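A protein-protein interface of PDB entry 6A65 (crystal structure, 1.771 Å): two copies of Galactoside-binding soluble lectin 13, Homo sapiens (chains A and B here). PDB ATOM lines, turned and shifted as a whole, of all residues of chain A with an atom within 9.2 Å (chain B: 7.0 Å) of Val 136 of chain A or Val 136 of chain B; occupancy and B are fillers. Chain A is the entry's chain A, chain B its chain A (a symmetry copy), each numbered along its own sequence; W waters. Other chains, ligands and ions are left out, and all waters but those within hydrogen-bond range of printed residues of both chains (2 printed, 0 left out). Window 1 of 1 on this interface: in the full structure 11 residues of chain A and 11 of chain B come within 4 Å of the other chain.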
ATOM      1  N   TYR A   7     -25.774   8.221  36.731  1.00  0.00           N
ATOM      2  CA  TYR A   7     -24.798   8.772  35.803  1.00  0.00           C
ATOM      3  C   TYR A   7     -24.720  10.274  36.048  1.00  0.00           C
ATOM      4  O   TYR A   7     -25.714  10.983  35.864  1.00  0.00           O
ATOM      5  CB  TYR A   7     -25.217   8.457  34.368  1.00  0.00           C
ATOM      6  CG  TYR A   7     -24.328   9.026  33.280  1.00  0.00           C
ATOM      7  CD1 TYR A   7     -23.051   8.534  33.071  1.00  0.00           C
ATOM      8  CD2 TYR A   7     -24.794  10.021  32.432  1.00  0.00           C
ATOM      9  CE1 TYR A   7     -22.246   9.045  32.068  1.00  0.00           C
ATOM     10  CE2 TYR A   7     -23.992  10.539  31.416  1.00  0.00           C
ATOM     11  CZ  TYR A   7     -22.724  10.044  31.244  1.00  0.00           C
ATOM     12  OH  TYR A   7     -21.932  10.568  30.239  1.00  0.00           O
ATOM     13  N   LEU A   9     -23.042  13.546  34.810  1.00  0.00           N
ATOM     14  CA  LEU A   9     -22.288  14.061  33.675  1.00  0.00           C
ATOM     15  C   LEU A   9     -22.012  15.541  33.857  1.00  0.00           C
ATOM     16  O   LEU A   9     -22.964  16.331  33.939  1.00  0.00           O
ATOM     17  CB  LEU A   9     -23.056  13.821  32.378  1.00  0.00           C
ATOM     18  CG  LEU A   9     -22.558  14.523  31.112  1.00  0.00           C
ATOM     19  CD1 LEU A   9     -21.238  13.937  30.582  1.00  0.00           C
ATOM     20  CD2 LEU A   9     -23.637  14.495  30.027  1.00  0.00           C
ATOM     21  N   PRO A  10     -20.754  15.969  33.929  1.00  0.00           N
ATOM     22  CA  PRO A  10     -20.471  17.408  33.865  1.00  0.00           C
ATOM     23  C   PRO A  10     -20.929  17.965  32.530  1.00  0.00           C
ATOM     24  O   PRO A  10     -20.690  17.377  31.473  1.00  0.00           O
ATOM     25  CB  PRO A  10     -18.945  17.482  34.024  1.00  0.00           C
ATOM     26  CG  PRO A  10     -18.546  16.139  34.583  1.00  0.00           C
ATOM     27  CD  PRO A  10     -19.525  15.161  34.036  1.00  0.00           C
ATOM     28  N   VAL A  11     -21.616  19.102  32.571  1.00  0.00           N
ATOM     29  CA  VAL A  11     -22.123  19.711  31.352  1.00  0.00           C
ATOM     30  C   VAL A  11     -21.883  21.209  31.397  1.00  0.00           C
ATOM     31  O   VAL A  11     -21.636  21.800  32.451  1.00  0.00           O
ATOM     32  CB  VAL A  11     -23.628  19.457  31.122  1.00  0.00           C
ATOM     33  CG1 VAL A  11     -23.937  17.984  31.026  1.00  0.00           C
ATOM     34  CG2 VAL A  11     -24.450  20.135  32.207  1.00  0.00           C
ATOM     35  N   SER A  12     -21.940  21.810  30.218  1.00  0.00           N
ATOM     36  CA  SER A  12     -22.115  23.247  30.064  1.00  0.00           C
ATOM     37  C   SER A  12     -23.308  23.446  29.146  1.00  0.00           C
ATOM     38  O   SER A  12     -23.336  22.899  28.039  1.00  0.00           O
ATOM     39  CB  SER A  12     -20.860  23.907  29.480  1.00  0.00           C
ATOM     40  OG  SER A  12     -20.999  25.312  29.485  1.00  0.00           O
ATOM     41  N   LEU A  13     -24.299  24.206  29.600  1.00  0.00           N
ATOM     42  CA  LEU A  13     -25.525  24.369  28.842  1.00  0.00           C
ATOM     43  C   LEU A  13     -25.694  25.821  28.442  1.00  0.00           C
ATOM     44  O   LEU A  13     -25.352  26.732  29.198  1.00  0.00           O
ATOM     45  CB  LEU A  13     -26.749  23.902  29.638  1.00  0.00           C
ATOM     46  CG  LEU A  13     -26.801  22.396  29.917  1.00  0.00           C
ATOM     47  CD1 LEU A  13     -28.142  21.998  30.483  1.00  0.00           C
ATOM     48  CD2 LEU A  13     -26.480  21.587  28.652  1.00  0.00           C
ATOM     49  N   SER A  14     -26.210  26.022  27.241  1.00  0.00           N
ATOM     50  CA  SER A  14     -26.542  27.350  26.758  1.00  0.00           C
ATOM     51  C   SER A  14     -27.829  27.240  25.968  1.00  0.00           C
ATOM     52  O   SER A  14     -28.254  26.146  25.601  1.00  0.00           O
ATOM     53  CB  SER A  14     -25.414  27.934  25.896  1.00  0.00           C
ATOM     54  OG  SER A  14     -25.260  27.195  24.698  1.00  0.00           O
ATOM     55  N   GLY A  16     -30.074  26.799  23.073  1.00  0.00           N
ATOM     56  CA  GLY A  16     -29.790  26.019  21.889  1.00  0.00           C
ATOM     57  C   GLY A  16     -29.208  24.641  22.146  1.00  0.00           C
ATOM     58  O   GLY A  16     -29.150  23.833  21.212  1.00  0.00           O
ATOM     59  N   SER A  17     -28.786  24.345  23.372  1.00  0.00           N
ATOM     60  CA  SER A  17     -28.267  23.018  23.680  1.00  0.00           C
ATOM     61  C   SER A  17     -29.387  21.986  23.702  1.00  0.00           C
ATOM     62  O   SER A  17     -30.555  22.295  23.956  1.00  0.00           O
ATOM     63  CB  SER A  17     -27.539  23.013  25.026  1.00  0.00           C
ATOM     64  OG  SER A  17     -26.627  24.083  25.135  1.00  0.00           O
ATOM     65  N   CYS A  18     -29.024  20.741  23.428  1.00  0.00           N
ATOM     66  CA  CYS A  18     -29.953  19.627  23.545  1.00  0.00           C
ATOM     67  C   CYS A  18     -29.277  18.531  24.345  1.00  0.00           C
ATOM     68  O   CYS A  18     -28.113  18.215  24.091  1.00  0.00           O
ATOM     69  CB  CYS A  18     -30.381  19.093  22.174  1.00  0.00           C
ATOM     70  SG  CYS A  18     -31.918  18.147  22.236  1.00  0.00           S
ATOM     71  N   VAL A  19     -29.990  17.978  25.325  1.00  0.00           N
ATOM     72  CA  VAL A  19     -29.530  16.814  26.067  1.00  0.00           C
ATOM     73  C   VAL A  19     -30.365  15.638  25.591  1.00  0.00           C
ATOM     74  O   VAL A  19     -31.594  15.644  25.727  1.00  0.00           O
ATOM     75  CB  VAL A  19     -29.653  17.017  27.584  1.00  0.00           C
ATOM     76  CG1 VAL A  19     -29.275  15.745  28.332  1.00  0.00           C
ATOM     77  CG2 VAL A  19     -28.780  18.176  28.028  1.00  0.00           C
ATOM     78  N   ILE A  20     -29.715  14.640  25.007  1.00  0.00           N
ATOM     79  CA  ILE A  20     -30.412  13.492  24.443  1.00  0.00           C
ATOM     80  C   ILE A  20     -30.036  12.263  25.258  1.00  0.00           C
ATOM     81  O   ILE A  20     -28.858  11.898  25.347  1.00  0.00           O
ATOM     82  CB  ILE A  20     -30.098  13.306  22.951  1.00  0.00           C
ATOM     83  CG1 ILE A  20     -30.369  14.611  22.197  1.00  0.00           C
ATOM     84  CG2 ILE A  20     -30.953  12.185  22.369  1.00  0.00           C
ATOM     85  CD1 ILE A  20     -29.114  15.357  21.785  1.00  0.00           C
ATOM     86  N   ILE A  21     -31.038  11.642  25.870  1.00  0.00           N
ATOM     87  CA  ILE A  21     -30.839  10.519  26.776  1.00  0.00           C
ATOM     88  C   ILE A  21     -31.500   9.302  26.152  1.00  0.00           C
ATOM     89  O   ILE A  21     -32.699   9.328  25.852  1.00  0.00           O
ATOM     90  CB  ILE A  21     -31.411  10.818  28.168  1.00  0.00           C
ATOM     91  CG1 ILE A  21     -30.545  11.867  28.867  1.00  0.00           C
ATOM     92  CG2 ILE A  21     -31.507   9.552  29.001  1.00  0.00           C
ATOM     93  CD1 ILE A  21     -31.305  12.648  29.941  1.00  0.00           C
ATOM     94  N   PHE A  39     -31.028  18.582  36.634  1.00  0.00           N
ATOM     95  CA  PHE A  39     -30.105  19.577  36.105  1.00  0.00           C
ATOM     96  C   PHE A  39     -29.507  20.309  37.298  1.00  0.00           C
ATOM     97  O   PHE A  39     -30.079  21.262  37.821  1.00  0.00           O
ATOM     98  CB  PHE A  39     -30.826  20.508  35.137  1.00  0.00           C
ATOM     99  CG  PHE A  39     -30.980  19.927  33.766  1.00  0.00           C
ATOM    100  CD1 PHE A  39     -31.027  18.555  33.581  1.00  0.00           C
ATOM    101  CD2 PHE A  39     -31.029  20.738  32.653  1.00  0.00           C
ATOM    102  CE1 PHE A  39     -31.157  18.019  32.312  1.00  0.00           C
ATOM    103  CE2 PHE A  39     -31.160  20.204  31.392  1.00  0.00           C
ATOM    104  CZ  PHE A  39     -31.221  18.856  31.216  1.00  0.00           C
ATOM    105  N   ILE A  92     -34.073  16.900  25.995  1.00  0.00           N
ATOM    106  CA  ILE A  92     -34.329  18.109  26.766  1.00  0.00           C
ATOM    107  C   ILE A  92     -33.660  19.255  26.021  1.00  0.00           C
ATOM    108  O   ILE A  92     -32.429  19.378  26.033  1.00  0.00           O
ATOM    109  CB  ILE A  92     -33.805  18.002  28.201  1.00  0.00           C
ATOM    110  CG1 ILE A  92     -34.483  16.823  28.923  1.00  0.00           C
ATOM    111  CG2 ILE A  92     -34.082  19.304  28.960  1.00  0.00           C
ATOM    112  CD1 ILE A  92     -33.707  16.345  30.115  1.00  0.00           C
ATOM    113  N   VAL A  94     -32.949  23.235  25.410  1.00  0.00           N
ATOM    114  CA  VAL A  94     -32.905  24.439  26.234  1.00  0.00           C
ATOM    115  C   VAL A  94     -33.209  25.621  25.325  1.00  0.00           C
ATOM    116  O   VAL A  94     -32.368  26.048  24.523  1.00  0.00           O
ATOM    117  CB  VAL A  94     -31.569  24.585  26.971  1.00  0.00           C
ATOM    118  CG1 VAL A  94     -30.474  24.342  26.064  1.00  0.00           C
ATOM    119  CG2 VAL A  94     -31.409  25.956  27.585  1.00  0.00           C
ATOM    120  N   VAL A 120     -26.389  25.496  34.919  1.00  0.00           N
ATOM    121  CA  VAL A 120     -26.347  24.042  35.061  1.00  0.00           C
ATOM    122  C   VAL A 120     -24.944  23.560  34.722  1.00  0.00           C
ATOM    123  O   VAL A 120     -24.426  23.846  33.635  1.00  0.00           O
ATOM    124  CB  VAL A 120     -27.390  23.371  34.153  1.00  0.00           C
ATOM    125  CG1 VAL A 120     -27.271  21.864  34.231  1.00  0.00           C
ATOM    126  CG2 VAL A 120     -28.807  23.837  34.533  1.00  0.00           C
ATOM    127  N   LYS A 121     -24.330  22.833  35.655  1.00  0.00           N
ATOM    128  CA  LYS A 121     -22.980  22.326  35.478  1.00  0.00           C
ATOM    129  C   LYS A 121     -22.911  20.812  35.495  1.00  0.00           C
ATOM    130  O   LYS A 121     -21.858  20.262  35.160  1.00  0.00           O
ATOM    131  CB  LYS A 121     -22.061  22.894  36.569  1.00  0.00           C
ATOM    132  CG  LYS A 121     -22.015  24.435  36.568  1.00  0.00           C
ATOM    133  CD  LYS A 121     -21.671  24.954  35.168  1.00  0.00           C
ATOM    134  CE  LYS A 121     -21.043  26.342  35.220  1.00  0.00           C
ATOM    135  NZ  LYS A 121     -21.168  27.070  33.917  1.00  0.00           N
ATOM    136  N   MET A 122     -23.989  20.124  35.874  1.00  0.00           N
ATOM    137  CA  MET A 122     -24.003  18.670  35.925  1.00  0.00           C
ATOM    138  C   MET A 122     -25.420  18.186  35.657  1.00  0.00           C
ATOM    139  O   MET A 122     -26.386  18.771  36.156  1.00  0.00           O
ATOM    140  CB  MET A 122     -23.503  18.159  37.281  1.00  0.00           C
ATOM    141  CG  MET A 122     -23.266  16.648  37.352  1.00  0.00           C
ATOM    142  SD  MET A 122     -24.704  15.810  38.046  1.00  0.00           S
ATOM    143  CE  MET A 122     -24.455  16.076  39.804  1.00  0.00           C
ATOM    144  N   VAL A 123     -25.542  17.135  34.850  1.00  0.00           N
ATOM    145  CA  VAL A 123     -26.815  16.461  34.635  1.00  0.00           C
ATOM    146  C   VAL A 123     -26.681  15.064  35.203  1.00  0.00           C
ATOM    147  O   VAL A 123     -25.751  14.332  34.848  1.00  0.00           O
ATOM    148  CB  VAL A 123     -27.223  16.395  33.154  1.00  0.00           C
ATOM    149  CG1 VAL A 123     -28.503  15.586  33.006  1.00  0.00           C
ATOM    150  CG2 VAL A 123     -27.434  17.799  32.587  1.00  0.00           C
ATOM    151  N   VAL A 125     -28.544  11.451  35.547  1.00  0.00           N
ATOM    152  CA  VAL A 125     -29.610  10.543  35.138  1.00  0.00           C
ATOM    153  C   VAL A 125     -29.628   9.389  36.134  1.00  0.00           C
ATOM    154  O   VAL A 125     -28.596   8.746  36.363  1.00  0.00           O
ATOM    155  CB  VAL A 125     -29.400  10.050  33.697  1.00  0.00           C
ATOM    156  CG1 VAL A 125     -30.589   9.222  33.235  1.00  0.00           C
ATOM    157  CG2 VAL A 125     -29.161  11.228  32.750  1.00  0.00           C
ATOM    158  N   SER A 133     -26.846   5.754  25.846  1.00  0.00           N
ATOM    159  CA  SER A 133     -26.047   6.909  25.468  1.00  0.00           C
ATOM    160  C   SER A 133     -26.644   8.186  26.043  1.00  0.00           C
ATOM    161  O   SER A 133     -27.855   8.278  26.287  1.00  0.00           O
ATOM    162  CB  SER A 133     -25.943   7.029  23.945  1.00  0.00           C
ATOM    163  OG  SER A 133     -27.231   7.122  23.365  1.00  0.00           O
ATOM    164  N   VAL A 134     -25.766   9.158  26.275  1.00  0.00           N
ATOM    165  CA  VAL A 134     -26.144  10.525  26.620  1.00  0.00           C
ATOM    166  C   VAL A 134     -25.282  11.466  25.794  1.00  0.00           C
ATOM    167  O   VAL A 134     -24.051  11.344  25.801  1.00  0.00           O
ATOM    168  CB  VAL A 134     -25.965  10.818  28.123  1.00  0.00           C
ATOM    169  CG1 VAL A 134     -26.268  12.278  28.418  1.00  0.00           C
ATOM    170  CG2 VAL A 134     -26.871   9.921  28.953  1.00  0.00           C
ATOM    171  N   CYS A 135     -25.923  12.401  25.089  1.00  0.00           N
ATOM    172  CA  CYS A 135     -25.249  13.375  24.235  1.00  0.00           C
ATOM    173  C   CYS A 135     -25.707  14.777  24.600  1.00  0.00           C
ATOM    174  O   CYS A 135     -26.893  15.002  24.864  1.00  0.00           O
ATOM    175  CB  CYS A 135     -25.555  13.144  22.764  1.00  0.00           C
ATOM    176  SG  CYS A 135     -25.010  11.583  22.116  1.00  0.00           S
ATOM    177  N   VAL A 136     -24.771  15.716  24.604  1.00  0.00           N
ATOM    178  CA  VAL A 136     -25.080  17.135  24.730  1.00  0.00           C
ATOM    179  C   VAL A 136     -24.680  17.784  23.417  1.00  0.00           C
ATOM    180  O   VAL A 136     -23.499  17.764  23.045  1.00  0.00           O
ATOM    181  CB  VAL A 136     -24.359  17.778  25.923  1.00  0.00           C
ATOM    182  CG1 VAL A 136     -24.713  19.263  26.005  1.00  0.00           C
ATOM    183  CG2 VAL A 136     -24.741  17.058  27.230  1.00  0.00           C
ATOM    184  N   CYS A 137     -25.667  18.317  22.699  1.00  0.00           N
ATOM    185  CA  CYS A 137     -25.484  18.837  21.354  1.00  0.00           C
ATOM    186  C   CYS A 137     -25.808  20.322  21.299  1.00  0.00           C
ATOM    187  O   CYS A 137     -26.574  20.838  22.114  1.00  0.00           O
ATOM    188  CB  CYS A 137     -26.390  18.111  20.349  1.00  0.00           C
ATOM    189  SG  CYS A 137     -26.020  16.391  20.075  1.00  0.00           S
ATOM    190  N   ASN A 138     -25.202  21.004  20.330  1.00  0.00           N
ATOM    191  CA  ASN A 138     -25.583  22.372  19.984  1.00  0.00           C
ATOM    192  C   ASN A 138     -25.612  22.511  18.470  1.00  0.00           C
ATOM    193  O   ASN A 138     -25.046  21.678  17.761  1.00  0.00           O
ATOM    194  CB  ASN A 138     -24.615  23.397  20.584  1.00  0.00           C
ATOM    195  CG  ASN A 138     -24.609  23.377  22.099  1.00  0.00           C
ATOM    196  OD1 ASN A 138     -25.347  24.123  22.748  1.00  0.00           O
ATOM    197  ND2 ASN A 138     -23.770  22.525  22.672  1.00  0.00           N
ATOM    198  N   LEU B   9     -16.386  25.688  22.632  1.00  0.00           N
ATOM    199  CA  LEU B   9     -17.362  24.929  23.403  1.00  0.00           C
ATOM    200  C   LEU B   9     -16.740  24.436  24.696  1.00  0.00           C
ATOM    201  O   LEU B   9     -15.768  23.669  24.648  1.00  0.00           O
ATOM    202  CB  LEU B   9     -17.882  23.751  22.583  1.00  0.00           C
ATOM    203  CG  LEU B   9     -18.711  22.687  23.306  1.00  0.00           C
ATOM    204  CD1 LEU B   9     -20.109  23.185  23.705  1.00  0.00           C
ATOM    205  CD2 LEU B   9     -18.809  21.419  22.455  1.00  0.00           C
ATOM    206  N   PRO B  10     -17.246  24.835  25.860  1.00  0.00           N
ATOM    207  CA  PRO B  10     -16.812  24.185  27.102  1.00  0.00           C
ATOM    208  C   PRO B  10     -17.184  22.714  27.072  1.00  0.00           C
ATOM    209  O   PRO B  10     -18.297  22.342  26.694  1.00  0.00           O
ATOM    210  CB  PRO B  10     -17.577  24.948  28.194  1.00  0.00           C
ATOM    211  CG  PRO B  10     -18.041  26.220  27.528  1.00  0.00           C
ATOM    212  CD  PRO B  10     -18.265  25.875  26.098  1.00  0.00           C
ATOM    213  N   VAL B  11     -16.240  21.860  27.454  1.00  0.00           N
ATOM    214  CA  VAL B  11     -16.483  20.427  27.441  1.00  0.00           C
ATOM    215  C   VAL B  11     -15.924  19.808  28.709  1.00  0.00           C
ATOM    216  O   VAL B  11     -15.100  20.395  29.414  1.00  0.00           O
ATOM    217  CB  VAL B  11     -15.858  19.712  26.224  1.00  0.00           C
ATOM    218  CG1 VAL B  11     -16.400  20.250  24.923  1.00  0.00           C
ATOM    219  CG2 VAL B  11     -14.342  19.799  26.281  1.00  0.00           C
ATOM    220  N   SER B  12     -16.410  18.609  28.995  1.00  0.00           N
ATOM    221  CA  SER B  12     -15.766  17.688  29.921  1.00  0.00           C
ATOM    222  C   SER B  12     -15.584  16.378  29.177  1.00  0.00           C
ATOM    223  O   SER B  12     -16.553  15.827  28.645  1.00  0.00           O
ATOM    224  CB  SER B  12     -16.605  17.486  31.189  1.00  0.00           C
ATOM    225  OG  SER B  12     -15.890  16.715  32.131  1.00  0.00           O
ATOM    226  N   LEU B  13     -14.352  15.883  29.119  1.00  0.00           N
ATOM    227  CA  LEU B  13     -14.060  14.692  28.343  1.00  0.00           C
ATOM    228  C   LEU B  13     -13.577  13.585  29.259  1.00  0.00           C
ATOM    229  O   LEU B  13     -12.866  13.833  30.233  1.00  0.00           O
ATOM    230  CB  LEU B  13     -13.010  14.967  27.259  1.00  0.00           C
ATOM    231  CG  LEU B  13     -13.468  15.913  26.143  1.00  0.00           C
ATOM    232  CD1 LEU B  13     -12.472  15.931  25.010  1.00  0.00           C
ATOM    233  CD2 LEU B  13     -14.867  15.536  25.635  1.00  0.00           C
ATOM    234  N   SER B  17     -15.799   9.216  25.596  1.00  0.00           N
ATOM    235  CA  SER B  17     -16.495  10.348  24.997  1.00  0.00           C
ATOM    236  C   SER B  17     -16.278  10.387  23.489  1.00  0.00           C
ATOM    237  O   SER B  17     -15.278   9.893  22.960  1.00  0.00           O
ATOM    238  CB  SER B  17     -16.027  11.668  25.614  1.00  0.00           C
ATOM    239  OG  SER B  17     -16.016  11.615  27.024  1.00  0.00           O
ATOM    240  N   CYS B  18     -17.235  10.979  22.788  1.00  0.00           N
ATOM    241  CA  CYS B  18     -17.104  11.214  21.358  1.00  0.00           C
ATOM    242  C   CYS B  18     -17.461  12.662  21.084  1.00  0.00           C
ATOM    243  O   CYS B  18     -18.463  13.157  21.604  1.00  0.00           O
ATOM    244  CB  CYS B  18     -18.008  10.284  20.542  1.00  0.00           C
ATOM    245  SG  CYS B  18     -17.479  10.120  18.823  1.00  0.00           S
ATOM    246  N   VAL B  19     -16.630  13.344  20.298  1.00  0.00           N
ATOM    247  CA  VAL B  19     -16.928  14.687  19.823  1.00  0.00           C
ATOM    248  C   VAL B  19     -17.279  14.559  18.350  1.00  0.00           C
ATOM    249  O   VAL B  19     -16.456  14.106  17.546  1.00  0.00           O
ATOM    250  CB  VAL B  19     -15.749  15.646  20.041  1.00  0.00           C
ATOM    251  CG1 VAL B  19     -16.042  17.011  19.432  1.00  0.00           C
ATOM    252  CG2 VAL B  19     -15.450  15.776  21.523  1.00  0.00           C
ATOM    253  N   ILE B  20     -18.502  14.926  17.992  1.00  0.00           N
ATOM    254  CA  ILE B  20     -18.980  14.781  16.623  1.00  0.00           C
ATOM    255  C   ILE B  20     -19.208  16.173  16.052  1.00  0.00           C
ATOM    256  O   ILE B  20     -20.010  16.951  16.581  1.00  0.00           O
ATOM    257  CB  ILE B  20     -20.248  13.917  16.548  1.00  0.00           C
ATOM    258  CG1 ILE B  20     -20.008  12.580  17.252  1.00  0.00           C
ATOM    259  CG2 ILE B  20     -20.633  13.675  15.093  1.00  0.00           C
ATOM    260  CD1 ILE B  20     -20.693  12.460  18.600  1.00  0.00           C
ATOM    261  N   VAL B 123     -13.270  22.777  23.606  1.00  0.00           N
ATOM    262  CA  VAL B 123     -12.960  22.391  22.236  1.00  0.00           C
ATOM    263  C   VAL B 123     -13.286  23.577  21.354  1.00  0.00           C
ATOM    264  O   VAL B 123     -14.402  24.104  21.401  1.00  0.00           O
ATOM    265  CB  VAL B 123     -13.740  21.151  21.767  1.00  0.00           C
ATOM    266  CG1 VAL B 123     -13.442  20.879  20.299  1.00  0.00           C
ATOM    267  CG2 VAL B 123     -13.365  19.927  22.602  1.00  0.00           C
ATOM    268  N   VAL B 134     -22.449  20.410  16.726  1.00  0.00           N
ATOM    269  CA  VAL B 134     -21.382  19.800  17.514  1.00  0.00           C
ATOM    270  C   VAL B 134     -22.024  19.102  18.701  1.00  0.00           C
ATOM    271  O   VAL B 134     -22.803  19.720  19.436  1.00  0.00           O
ATOM    272  CB  VAL B 134     -20.351  20.839  18.000  1.00  0.00           C
ATOM    273  CG1 VAL B 134     -19.320  20.180  18.901  1.00  0.00           C
ATOM    274  CG2 VAL B 134     -19.660  21.500  16.816  1.00  0.00           C
ATOM    275  N   CYS B 135     -21.697  17.822  18.890  1.00  0.00           N
ATOM    276  CA  CYS B 135     -22.232  17.001  19.972  1.00  0.00           C
ATOM    277  C   CYS B 135     -21.088  16.353  20.735  1.00  0.00           C
ATOM    278  O   CYS B 135     -20.108  15.902  20.132  1.00  0.00           O
ATOM    279  CB  CYS B 135     -23.139  15.898  19.450  1.00  0.00           C
ATOM    280  SG  CYS B 135     -24.594  16.456  18.601  1.00  0.00           S
ATOM    281  N   VAL B 136     -21.220  16.298  22.053  1.00  0.00           N
ATOM    282  CA  VAL B 136     -20.317  15.534  22.903  1.00  0.00           C
ATOM    283  C   VAL B 136     -21.141  14.417  23.518  1.00  0.00           C
ATOM    284  O   VAL B 136     -22.099  14.682  24.256  1.00  0.00           O
ATOM    285  CB  VAL B 136     -19.657  16.409  23.979  1.00  0.00           C
ATOM    286  CG1 VAL B 136     -18.728  15.557  24.843  1.00  0.00           C
ATOM    287  CG2 VAL B 136     -18.879  17.565  23.323  1.00  0.00           C
ATOM    288  N   CYS B 137     -20.798  13.176  23.178  1.00  0.00           N
ATOM    289  CA  CYS B 137     -21.574  12.004  23.549  1.00  0.00           C
ATOM    290  C   CYS B 137     -20.753  11.065  24.420  1.00  0.00           C
ATOM    291  O   CYS B 137     -19.522  11.060  24.368  1.00  0.00           O
ATOM    292  CB  CYS B 137     -22.035  11.226  22.307  1.00  0.00           C
ATOM    293  SG  CYS B 137     -23.208  12.062  21.261  1.00  0.00           S
ATOM    294  N   ASN B 138     -21.456  10.277  25.230  1.00  0.00           N
ATOM    295  CA  ASN B 138     -20.849   9.158  25.948  1.00  0.00           C
ATOM    296  C   ASN B 138     -21.783   7.959  25.880  1.00  0.00           C
ATOM    297  O   ASN B 138     -22.966   8.113  25.575  1.00  0.00           O
ATOM    298  CB  ASN B 138     -20.562   9.513  27.410  1.00  0.00           C
ATOM    299  CG  ASN B 138     -19.561  10.641  27.551  1.00  0.00           C
ATOM    300  OD1 ASN B 138     -18.355  10.411  27.671  1.00  0.00           O
ATOM    301  ND2 ASN B 138     -20.056  11.871  27.543  1.00  0.00           N
HETATM  302  O   HOH W   1     -21.934  21.449  21.236  1.00  0.00           O
HETATM  303  O   HOH W   2     -22.587  12.183  27.836  1.00  0.00           O
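Along chain A the printed residues that touch a printed residue of chain B span positions 7 to 138.
Of the 15 printed residues of chain B, 8 touch a printed residue of chain A.
Hydrophobic or aromatic side chains of chain B within 4 Å of the printed part of chain A: Leu 9 and Pro 10.
Along chain B the printed residues that touch a printed residue of chain A span positions 9 to 138.
Among the printed residues, no Asp or Glu carboxylate lies within 4 Å of a Lys or Arg side-chain nitrogen of the other chain.
Of chain B, only Cys 135 (3.4 Å) and Val 136 (2.9 Å) come within 4 Å of Val 136 of chain A.
Of chain A, only Cys 135 (3.4 Å) and Val 136 (2.9 Å) come within 4 Å of Val 136 of chain B.
Cys 135 of chain B touches two residues of chain A.
Cys 137 of chain B touches just these residues of chain A: Val 134 and Cys 135.
Of the printed residues of chain B, Cys 137 of chain A touches Val 134 (3.4 Å) and Cys 135 (2.1 Å).
Of the printed residues of chain B, Pro 10 of chain A touches Ser 12 (3.7 Å).
Of the printed residues of chain B, Ser 12 of chain A touches Pro 10 (3.7 Å).
Of the printed residues of chain B, Leu 9 of chain A touches Asn 138.
Val 94 of chain A touches none of the printed residues of chain B.
The nearest residue of chain B that does not touch Val 136 of chain A is Val 134 of chain B (4.2 Å).
The nearest residue of chain A that does not touch Val 136 of chain B is Val 134 of chain A (4.2 Å).
The nearest printed residue of chain B that does not touch Pro 10 of chain A is Val 11 of chain B (6.0 Å).
Water W1 lies within hydrogen-bond range of ND2 of Asn 138 of chain A (2.6 Å) and O of Val 134 of chain B (2.6 Å).
Water W2 lies within hydrogen-bond range of the side-chain amide nitrogen of Asn 138 of chain B (2.6 Å), the backbone carbonyl oxygen of Val 134 of chain A (2.6 Å) and the side-chain hydroxyl of Tyr 7 of chain A (3.0 Å).
Val 134 of chain A touches Cys 137 of chain B, and with the chains exchanged Cys 137 of chain A touches Val 134 of chain B.
Cys 135 of chain A touches Val 136 of chain B, and with the chains exchanged Val 136 of chain A touches Cys 135 of chain B.
15 positions are printed for both chains.
O of Val 134 of chain A lies within hydrogen-bond range of N of Asn 138 of chain B (2.9 Å).
The side-chain sulfur (SG) of Cys 137 of chain B forms a disulfide with the side-chain sulfur (SG) of Cys 135 of chain A (2.1 Å).
N of Val 136 of chain A is in hydrogen-bond range of O of Val 136 of chain B (2.9 Å).
The side-chain sulfur of Cys 137 of chain A forms a disulfide with the side-chain sulfur of Cys 135 of chain B.
O of Val 134 of chain B sits at hydrogen-bond distance from N of Asn 138 of chain A, 2.9 Å away.
O of Tyr 7 of chain A is in hydrogen-bond range of N of Val 125 of chain A, 2.9 Å away.
OD1 of Asn 138 of chain B lies within hydrogen-bond range of OG of Ser 17 of chain B (2.7 Å).
O of Cys 135 of chain B lies within hydrogen-bond range of N of Ile 20 of chain B (2.8 Å).
Among the printed residues, pairs that only touch across the chains: Tyr 7 of chain A with Asn 138 of chain B, Leu 9 of chain A with Asn 138 of chain B, Pro 10 of chain A with Ser 12 of chain B, Ser 12 of chain A with Pro 10 of chain B, Ser 133 of chain A with Asn 138 of chain B, Val 134 of chain A with Cys 137 of chain B, Cys 135 of chain A with Val 136 of chain B, Val 136 of chain A with Cys 135 of chain B, Cys 137 of chain A with Val 134 of chain B and Asn 138 of chain A with Leu 9 of chain B.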
